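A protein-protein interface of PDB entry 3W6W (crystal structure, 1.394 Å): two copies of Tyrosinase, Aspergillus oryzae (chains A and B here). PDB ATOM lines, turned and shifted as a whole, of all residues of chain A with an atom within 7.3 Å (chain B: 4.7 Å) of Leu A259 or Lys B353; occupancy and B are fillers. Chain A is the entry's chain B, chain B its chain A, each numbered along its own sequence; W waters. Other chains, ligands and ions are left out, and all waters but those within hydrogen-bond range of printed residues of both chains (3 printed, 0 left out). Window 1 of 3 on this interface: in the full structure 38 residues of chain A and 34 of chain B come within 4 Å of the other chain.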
ATOM      1  N   GLY A 165      -4.811  37.791   2.738  1.00  0.00           N
ATOM      2  CA  GLY A 165      -3.529  38.324   2.308  1.00  0.00           C
ATOM      3  C   GLY A 165      -3.244  38.100   0.835  1.00  0.00           C
ATOM      4  O   GLY A 165      -4.054  37.516   0.115  1.00  0.00           O
ATOM      5  N   GLU A 167      -1.119  36.536  -2.422  1.00  0.00           N
ATOM      6  CA  GLU A 167      -0.418  35.303  -2.768  1.00  0.00           C
ATOM      7  C   GLU A 167      -0.239  35.165  -4.267  1.00  0.00           C
ATOM      8  O   GLU A 167      -0.943  35.793  -5.053  1.00  0.00           O
ATOM      9  CB  GLU A 167      -1.162  34.074  -2.227  1.00  0.00           C
ATOM     10  CG  GLU A 167      -2.365  33.659  -3.054  1.00  0.00           C
ATOM     11  CD  GLU A 167      -2.997  32.357  -2.581  1.00  0.00           C
ATOM     12  OE1 GLU A 167      -4.026  31.957  -3.172  1.00  0.00           O
ATOM     13  OE2 GLU A 167      -2.465  31.737  -1.631  1.00  0.00           O
ATOM     14  N   ARG A 169      -0.453  32.793  -7.665  1.00  0.00           N
ATOM     15  CA  ARG A 169      -1.428  31.783  -8.082  1.00  0.00           C
ATOM     16  C   ARG A 169      -1.252  31.375  -9.528  1.00  0.00           C
ATOM     17  O   ARG A 169      -0.842  32.180 -10.363  1.00  0.00           O
ATOM     18  CB  ARG A 169      -2.868  32.319  -7.973  1.00  0.00           C
ATOM     19  CG  ARG A 169      -3.367  32.637  -6.564  1.00  0.00           C
ATOM     20  CD  ARG A 169      -4.834  32.987  -6.584  1.00  0.00           C
ATOM     21  NE  ARG A 169      -5.341  33.157  -5.227  1.00  0.00           N
ATOM     22  CZ  ARG A 169      -6.542  33.642  -4.940  1.00  0.00           C
ATOM     23  NH1 ARG A 169      -7.357  34.032  -5.915  1.00  0.00           N
ATOM     24  NH2 ARG A 169      -6.921  33.752  -3.674  1.00  0.00           N
ATOM     25  N   LEU A 170      -1.595  30.126  -9.811  1.00  0.00           N
ATOM     26  CA  LEU A 170      -1.876  29.673 -11.171  1.00  0.00           C
ATOM     27  C   LEU A 170      -2.910  30.597 -11.800  1.00  0.00           C
ATOM     28  O   LEU A 170      -3.784  31.142 -11.082  1.00  0.00           O
ATOM     29  CB  LEU A 170      -2.456  28.254 -11.140  1.00  0.00           C
ATOM     30  CG  LEU A 170      -1.485  27.089 -10.915  1.00  0.00           C
ATOM     31  CD1 LEU A 170      -2.243  25.765 -10.777  1.00  0.00           C
ATOM     32  CD2 LEU A 170      -0.461  27.021 -12.030  1.00  0.00           C
ATOM     33  N   THR A 175      -7.360  27.037 -13.837  1.00  0.00           N
ATOM     34  CA  THR A 175      -8.058  26.358 -12.751  1.00  0.00           C
ATOM     35  C   THR A 175      -9.546  26.080 -13.056  1.00  0.00           C
ATOM     36  O   THR A 175     -10.280  25.597 -12.211  1.00  0.00           O
ATOM     37  CB  THR A 175      -7.936  27.127 -11.421  1.00  0.00           C
ATOM     38  OG1 THR A 175      -8.733  28.329 -11.478  1.00  0.00           O
ATOM     39  CG2 THR A 175      -6.484  27.492 -11.154  1.00  0.00           C
ATOM     40  N   TYR A 240       0.193  17.091  -9.787  1.00  0.00           N
ATOM     41  CA  TYR A 240       0.186  16.389  -8.492  1.00  0.00           C
ATOM     42  C   TYR A 240      -0.701  15.152  -8.436  1.00  0.00           C
ATOM     43  O   TYR A 240      -0.981  14.653  -7.351  1.00  0.00           O
ATOM     44  CB  TYR A 240      -0.189  17.332  -7.332  1.00  0.00           C
ATOM     45  CG  TYR A 240       0.856  18.382  -7.054  1.00  0.00           C
ATOM     46  CD1 TYR A 240       0.840  19.593  -7.743  1.00  0.00           C
ATOM     47  CD2 TYR A 240       1.851  18.163  -6.110  1.00  0.00           C
ATOM     48  CE1 TYR A 240       1.804  20.551  -7.518  1.00  0.00           C
ATOM     49  CE2 TYR A 240       2.817  19.130  -5.865  1.00  0.00           C
ATOM     50  CZ  TYR A 240       2.776  20.320  -6.573  1.00  0.00           C
ATOM     51  OH  TYR A 240       3.720  21.287  -6.347  1.00  0.00           O
ATOM     52  N   GLN A 256      -6.257  18.069 -11.752  1.00  0.00           N
ATOM     53  CA  GLN A 256      -5.436  19.268 -11.640  1.00  0.00           C
ATOM     54  C   GLN A 256      -5.550  19.783 -10.208  1.00  0.00           C
ATOM     55  O   GLN A 256      -6.511  20.475  -9.837  1.00  0.00           O
ATOM     56  CB  GLN A 256      -5.922  20.347 -12.615  1.00  0.00           C
ATOM     57  CG  GLN A 256      -6.222  19.842 -14.029  1.00  0.00           C
ATOM     58  CD  GLN A 256      -5.046  19.128 -14.668  1.00  0.00           C
ATOM     59  OE1 GLN A 256      -3.905  19.602 -14.616  1.00  0.00           O
ATOM     60  NE2 GLN A 256      -5.321  17.980 -15.285  1.00  0.00           N
ATOM     61  N   ASN A 257      -4.580  19.437  -9.388  1.00  0.00           N
ATOM     62  CA  ASN A 257      -4.658  19.869  -8.013  1.00  0.00           C
ATOM     63  C   ASN A 257      -4.136  21.285  -7.938  1.00  0.00           C
ATOM     64  O   ASN A 257      -3.004  21.504  -7.508  1.00  0.00           O
ATOM     65  CB  ASN A 257      -3.837  18.943  -7.121  1.00  0.00           C
ATOM     66  CG  ASN A 257      -4.141  19.159  -5.656  1.00  0.00           C
ATOM     67  OD1 ASN A 257      -4.554  20.250  -5.271  1.00  0.00           O
ATOM     68  ND2 ASN A 257      -3.937  18.131  -4.833  1.00  0.00           N
ATOM     69  N   TRP A 258      -4.950  22.244  -8.383  1.00  0.00           N
ATOM     70  CA  TRP A 258      -4.435  23.594  -8.533  1.00  0.00           C
ATOM     71  C   TRP A 258      -4.192  24.279  -7.193  1.00  0.00           C
ATOM     72  O   TRP A 258      -3.312  25.124  -7.092  1.00  0.00           O
ATOM     73  CB  TRP A 258      -5.304  24.443  -9.477  1.00  0.00           C
ATOM     74  CG  TRP A 258      -6.708  24.689  -9.028  1.00  0.00           C
ATOM     75  CD1 TRP A 258      -7.838  24.007  -9.418  1.00  0.00           C
ATOM     76  CD2 TRP A 258      -7.158  25.704  -8.121  1.00  0.00           C
ATOM     77  NE1 TRP A 258      -8.939  24.527  -8.802  1.00  0.00           N
ATOM     78  CE2 TRP A 258      -8.553  25.568  -7.996  1.00  0.00           C
ATOM     79  CE3 TRP A 258      -6.515  26.719  -7.399  1.00  0.00           C
ATOM     80  CZ2 TRP A 258      -9.312  26.409  -7.193  1.00  0.00           C
ATOM     81  CZ3 TRP A 258      -7.273  27.545  -6.576  1.00  0.00           C
ATOM     82  CH2 TRP A 258      -8.657  27.388  -6.484  1.00  0.00           C
ATOM     83  N   LEU A 259      -4.955  23.908  -6.168  1.00  0.00           N
ATOM     84  CA  LEU A 259      -4.740  24.460  -4.831  1.00  0.00           C
ATOM     85  C   LEU A 259      -3.381  23.995  -4.305  1.00  0.00           C
ATOM     86  O   LEU A 259      -2.655  24.765  -3.680  1.00  0.00           O
ATOM     87  CB  LEU A 259      -5.867  24.036  -3.888  1.00  0.00           C
ATOM     88  CG  LEU A 259      -6.194  24.883  -2.655  1.00  0.00           C
ATOM     89  CD1 LEU A 259      -6.636  26.300  -3.011  1.00  0.00           C
ATOM     90  CD2 LEU A 259      -7.281  24.200  -1.848  1.00  0.00           C
ATOM     91  N   ARG A 260      -3.034  22.739  -4.563  1.00  0.00           N
ATOM     92  CA  ARG A 260      -1.719  22.247  -4.140  1.00  0.00           C
ATOM     93  C   ARG A 260      -0.588  22.952  -4.881  1.00  0.00           C
ATOM     94  O   ARG A 260       0.451  23.253  -4.300  1.00  0.00           O
ATOM     95  CB  ARG A 260      -1.594  20.734  -4.336  1.00  0.00           C
ATOM     96  CG  ARG A 260      -0.195  20.179  -4.042  1.00  0.00           C
ATOM     97  CD  ARG A 260       0.112  20.288  -2.553  1.00  0.00           C
ATOM     98  NE  ARG A 260       1.457  19.837  -2.201  1.00  0.00           N
ATOM     99  CZ  ARG A 260       2.518  20.631  -2.092  1.00  0.00           C
ATOM    100  NH1 ARG A 260       2.431  21.929  -2.352  1.00  0.00           N
ATOM    101  NH2 ARG A 260       3.688  20.129  -1.725  1.00  0.00           N
ATOM    102  N   ALA A 261      -0.767  23.168  -6.182  1.00  0.00           N
ATOM    103  CA  ALA A 261       0.243  23.884  -6.957  1.00  0.00           C
ATOM    104  C   ALA A 261       0.406  25.310  -6.447  1.00  0.00           C
ATOM    105  O   ALA A 261       1.525  25.797  -6.330  1.00  0.00           O
ATOM    106  CB  ALA A 261      -0.098  23.883  -8.452  1.00  0.00           C
ATOM    107  N   ASN A 262      -0.710  25.976  -6.148  1.00  0.00           N
ATOM    108  CA  ASN A 262      -0.627  27.322  -5.600  1.00  0.00           C
ATOM    109  C   ASN A 262       0.157  27.339  -4.300  1.00  0.00           C
ATOM    110  O   ASN A 262       0.974  28.239  -4.070  1.00  0.00           O
ATOM    111  CB  ASN A 262      -2.025  27.890  -5.343  1.00  0.00           C
ATOM    112  CG  ASN A 262      -2.692  28.413  -6.596  1.00  0.00           C
ATOM    113  OD1 ASN A 262      -2.150  28.312  -7.701  1.00  0.00           O
ATOM    114  ND2 ASN A 262      -3.891  28.980  -6.420  1.00  0.00           N
ATOM    115  N   LEU A 263      -0.055  26.323  -3.466  1.00  0.00           N
ATOM    116  CA  LEU A 263       0.678  26.226  -2.211  1.00  0.00           C
ATOM    117  C   LEU A 263       2.178  26.122  -2.477  1.00  0.00           C
ATOM    118  O   LEU A 263       2.970  26.833  -1.860  1.00  0.00           O
ATOM    119  CB  LEU A 263       0.198  25.032  -1.388  1.00  0.00           C
ATOM    120  CG  LEU A 263       1.041  24.752  -0.135  1.00  0.00           C
ATOM    121  CD1 LEU A 263       1.001  25.937   0.843  1.00  0.00           C
ATOM    122  CD2 LEU A 263       0.550  23.471   0.534  1.00  0.00           C
ATOM    123  N   ALA A 264       2.561  25.246  -3.397  1.00  0.00           N
ATOM    124  CA  ALA A 264       3.981  25.089  -3.734  1.00  0.00           C
ATOM    125  C   ALA A 264       4.560  26.404  -4.287  1.00  0.00           C
ATOM    126  O   ALA A 264       5.683  26.807  -3.958  1.00  0.00           O
ATOM    127  CB  ALA A 264       4.167  23.948  -4.740  1.00  0.00           C
ATOM    128  N   LEU A 265       3.796  27.074  -5.144  1.00  0.00           N
ATOM    129  CA  LEU A 265       4.234  28.338  -5.735  1.00  0.00           C
ATOM    130  C   LEU A 265       4.506  29.424  -4.701  1.00  0.00           C
ATOM    131  O   LEU A 265       5.290  30.352  -4.953  1.00  0.00           O
ATOM    132  CB  LEU A 265       3.182  28.831  -6.730  1.00  0.00           C
ATOM    133  CG  LEU A 265       3.099  28.034  -8.029  1.00  0.00           C
ATOM    134  CD1 LEU A 265       1.827  28.369  -8.789  1.00  0.00           C
ATOM    135  CD2 LEU A 265       4.344  28.282  -8.889  1.00  0.00           C
ATOM    136  N   ASN A 266       3.862  29.314  -3.544  1.00  0.00           N
ATOM    137  CA  ASN A 266       4.061  30.272  -2.469  1.00  0.00           C
ATOM    138  C   ASN A 266       5.080  29.810  -1.442  1.00  0.00           C
ATOM    139  O   ASN A 266       5.091  30.293  -0.319  1.00  0.00           O
ATOM    140  CB  ASN A 266       2.726  30.599  -1.787  1.00  0.00           C
ATOM    141  CG  ASN A 266       1.865  31.504  -2.632  1.00  0.00           C
ATOM    142  OD1 ASN A 266       2.040  32.721  -2.607  1.00  0.00           O
ATOM    143  ND2 ASN A 266       0.954  30.924  -3.412  1.00  0.00           N
ATOM    144  N   LEU B 243     -14.354  27.834  -2.676  1.00  0.00           N
ATOM    145  CA  LEU B 243     -13.626  28.674  -1.730  1.00  0.00           C
ATOM    146  C   LEU B 243     -13.848  30.135  -2.084  1.00  0.00           C
ATOM    147  O   LEU B 243     -13.867  30.518  -3.255  1.00  0.00           O
ATOM    148  CB  LEU B 243     -12.111  28.376  -1.757  1.00  0.00           C
ATOM    149  CG  LEU B 243     -11.569  27.083  -1.148  1.00  0.00           C
ATOM    150  CD1 LEU B 243     -11.803  25.905  -2.092  1.00  0.00           C
ATOM    151  CD2 LEU B 243     -10.074  27.222  -0.816  1.00  0.00           C
ATOM    152  N   TYR B 246     -11.814  33.377  -4.869  1.00  0.00           N
ATOM    153  CA  TYR B 246     -11.386  32.922  -6.191  1.00  0.00           C
ATOM    154  C   TYR B 246     -12.452  33.400  -7.156  1.00  0.00           C
ATOM    155  O   TYR B 246     -13.590  33.674  -6.746  1.00  0.00           O
ATOM    156  CB  TYR B 246     -11.205  31.395  -6.253  1.00  0.00           C
ATOM    157  CG  TYR B 246     -10.111  30.946  -5.328  1.00  0.00           C
ATOM    158  CD1 TYR B 246      -8.780  30.929  -5.738  1.00  0.00           C
ATOM    159  CD2 TYR B 246     -10.403  30.600  -4.012  1.00  0.00           C
ATOM    160  CE1 TYR B 246      -7.773  30.550  -4.859  1.00  0.00           C
ATOM    161  CE2 TYR B 246      -9.414  30.222  -3.133  1.00  0.00           C
ATOM    162  CZ  TYR B 246      -8.104  30.199  -3.567  1.00  0.00           C
ATOM    163  OH  TYR B 246      -7.126  29.831  -2.673  1.00  0.00           O
ATOM    164  N   HIS B 350      -3.295  32.041   5.700  1.00  0.00           N
ATOM    165  CA  HIS B 350      -2.986  30.612   5.679  1.00  0.00           C
ATOM    166  C   HIS B 350      -2.499  30.188   4.296  1.00  0.00           C
ATOM    167  O   HIS B 350      -3.249  30.285   3.327  1.00  0.00           O
ATOM    168  CB  HIS B 350      -4.225  29.783   6.054  1.00  0.00           C
ATOM    169  CG  HIS B 350      -4.887  30.230   7.317  1.00  0.00           C
ATOM    170  ND1 HIS B 350      -4.453  29.836   8.564  1.00  0.00           N
ATOM    171  CD2 HIS B 350      -5.924  31.078   7.529  1.00  0.00           C
ATOM    172  CE1 HIS B 350      -5.206  30.404   9.490  1.00  0.00           C
ATOM    173  NE2 HIS B 350      -6.102  31.167   8.887  1.00  0.00           N
ATOM    174  N   ASP B 351      -1.256  29.719   4.185  1.00  0.00           N
ATOM    175  CA  ASP B 351      -0.756  29.241   2.900  1.00  0.00           C
ATOM    176  C   ASP B 351      -1.363  27.891   2.547  1.00  0.00           C
ATOM    177  O   ASP B 351      -1.871  27.705   1.450  1.00  0.00           O
ATOM    178  CB  ASP B 351       0.765  29.144   2.907  1.00  0.00           C
ATOM    179  CG  ASP B 351       1.430  30.498   2.884  1.00  0.00           C
ATOM    180  OD1 ASP B 351       0.998  31.360   2.089  1.00  0.00           O
ATOM    181  OD2 ASP B 351       2.375  30.699   3.664  1.00  0.00           O
ATOM    182  N   LEU B 352      -1.327  26.954   3.494  1.00  0.00           N
ATOM    183  CA  LEU B 352      -2.005  25.667   3.302  1.00  0.00           C
ATOM    184  C   LEU B 352      -3.474  25.875   3.592  1.00  0.00           C
ATOM    185  O   LEU B 352      -3.850  26.238   4.704  1.00  0.00           O
ATOM    186  CB  LEU B 352      -1.426  24.575   4.208  1.00  0.00           C
ATOM    187  CG  LEU B 352      -2.196  23.251   4.261  1.00  0.00           C
ATOM    188  CD1 LEU B 352      -2.233  22.574   2.903  1.00  0.00           C
ATOM    189  CD2 LEU B 352      -1.601  22.328   5.315  1.00  0.00           C
ATOM    190  N   LYS B 353      -4.290  25.661   2.576  1.00  0.00           N
ATOM    191  CA  LYS B 353      -5.713  25.908   2.696  1.00  0.00           C
ATOM    192  C   LYS B 353      -6.466  24.586   2.789  1.00  0.00           C
ATOM    193  O   LYS B 353      -6.518  23.803   1.840  1.00  0.00           O
ATOM    194  CB  LYS B 353      -6.182  26.779   1.530  1.00  0.00           C
ATOM    195  CG  LYS B 353      -5.403  28.094   1.442  1.00  0.00           C
ATOM    196  CD  LYS B 353      -5.737  28.877   0.188  1.00  0.00           C
ATOM    197  CE  LYS B 353      -4.809  30.061  -0.003  1.00  0.00           C
ATOM    198  NZ  LYS B 353      -4.864  31.021   1.117  1.00  0.00           N
ATOM    199  N   LEU B 354      -7.046  24.345   3.958  1.00  0.00           N
ATOM    200  CA  LEU B 354      -7.679  23.069   4.246  1.00  0.00           C
ATOM    201  C   LEU B 354      -9.191  23.162   4.171  1.00  0.00           C
ATOM    202  O   LEU B 354      -9.884  22.153   4.300  1.00  0.00           O
ATOM    203  CB  LEU B 354      -7.235  22.582   5.624  1.00  0.00           C
ATOM    204  CG  LEU B 354      -5.743  22.257   5.686  1.00  0.00           C
ATOM    205  CD1 LEU B 354      -5.215  22.274   7.122  1.00  0.00           C
ATOM    206  CD2 LEU B 354      -5.512  20.919   5.032  1.00  0.00           C
ATOM    207  N   TRP B 355      -9.694  24.370   3.948  1.00  0.00           N
ATOM    208  CA  TRP B 355     -11.135  24.568   3.800  1.00  0.00           C
ATOM    209  C   TRP B 355     -11.549  24.406   2.350  1.00  0.00           C
ATOM    210  O   TRP B 355     -10.759  23.969   1.525  1.00  0.00           O
ATOM    211  CB  TRP B 355     -11.577  25.930   4.357  1.00  0.00           C
ATOM    212  CG  TRP B 355     -11.015  27.143   3.677  1.00  0.00           C
ATOM    213  CD1 TRP B 355     -11.621  27.902   2.716  1.00  0.00           C
ATOM    214  CD2 TRP B 355      -9.736  27.751   3.920  1.00  0.00           C
ATOM    215  NE1 TRP B 355     -10.807  28.945   2.347  1.00  0.00           N
ATOM    216  CE2 TRP B 355      -9.642  28.878   3.074  1.00  0.00           C
ATOM    217  CE3 TRP B 355      -8.672  27.462   4.784  1.00  0.00           C
ATOM    218  CZ2 TRP B 355      -8.524  29.708   3.055  1.00  0.00           C
ATOM    219  CZ3 TRP B 355      -7.562  28.286   4.765  1.00  0.00           C
ATOM    220  CH2 TRP B 355      -7.496  29.401   3.914  1.00  0.00           C
HETATM  221  O   HOH W   1      -4.616  29.328  -3.550  1.00  0.00           O
HETATM  222  O   HOH W   2       2.444  33.697   0.012  1.00  0.00           O
HETATM  223  O   HOH W   3      -1.340  28.728  -1.280  1.00  0.00           O
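The side-chain amino group (NZ) of Lys B353 is in salt-bridge range of the side-chain carboxylate (OE2) of Glu A167 (3.7 Å).
The guanidinium group (NE) of Arg A169 is in salt-bridge range of the side-chain carboxylate (OE1) of Glu A167 (2.7 Å).
OD1 of Asn A262 lies close to O of Trp A258, 3.4 Å away.
NZ of Lys B353 sits at hydrogen-bond distance from O of His B350 (2.8 Å).
Among the printed residues, pairs that only touch across the chains: Glu A167 with Tyr B246, Arg A169 with Tyr B246, Trp A258 with Tyr B246, Leu A259 with Tyr B246, Leu A259 with Lys B353, Leu A263 with Asp B351 and Leu A263 with Leu B352.
Printed residues of chain B within 4 Å of Leu A259: Tyr B246 (3.6 Å) and Lys B353 (3.8 Å).
Of the printed residues of chain A, Lys B353 touches Glu A167 (3.3 Å) and Leu A259 (3.8 Å).
Of the printed residues of chain A, Asp B351 touches Leu A263.
Of the printed residues of chain B, Trp A258 touches Tyr B246 (3.5 Å).
Of the printed residues of chain A, Tyr B246 touches Glu A167 (3.8 Å), Arg A169 (3.3 Å), Trp A258 (3.5 Å) and Leu A259 (3.6 Å).
Printed residues of chain B within 4 Å of Arg A169: Tyr B246.
Asn A262 touches none of the printed residues of chain B.
Leu B354 touches none of the printed residues of chain A.
The nearest printed residue of chain B that does not touch Leu A259 is Leu B243 (4.2 Å).
Of the 8 printed residues of chain B, 4 touch a printed residue of chain A.
Among the printed residues, 8 pairs touch across the chains.
No position is printed for both chains.
Water W1 lies within hydrogen-bond range of the side-chain hydroxyl (OH) of Tyr B246, the side-chain carboxylate (OE1) of Glu A167 and the side-chain amide nitrogen (ND2) of Asn A262.
Water W2 bridges the side-chain amide oxygen (OD1) of Asn A266 and the side-chain carboxylate (OD1) of Asp B351.
Water W3 lies within hydrogen-bond range of O of Asp B351, OE2 of Glu A167 and N of Leu A263.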
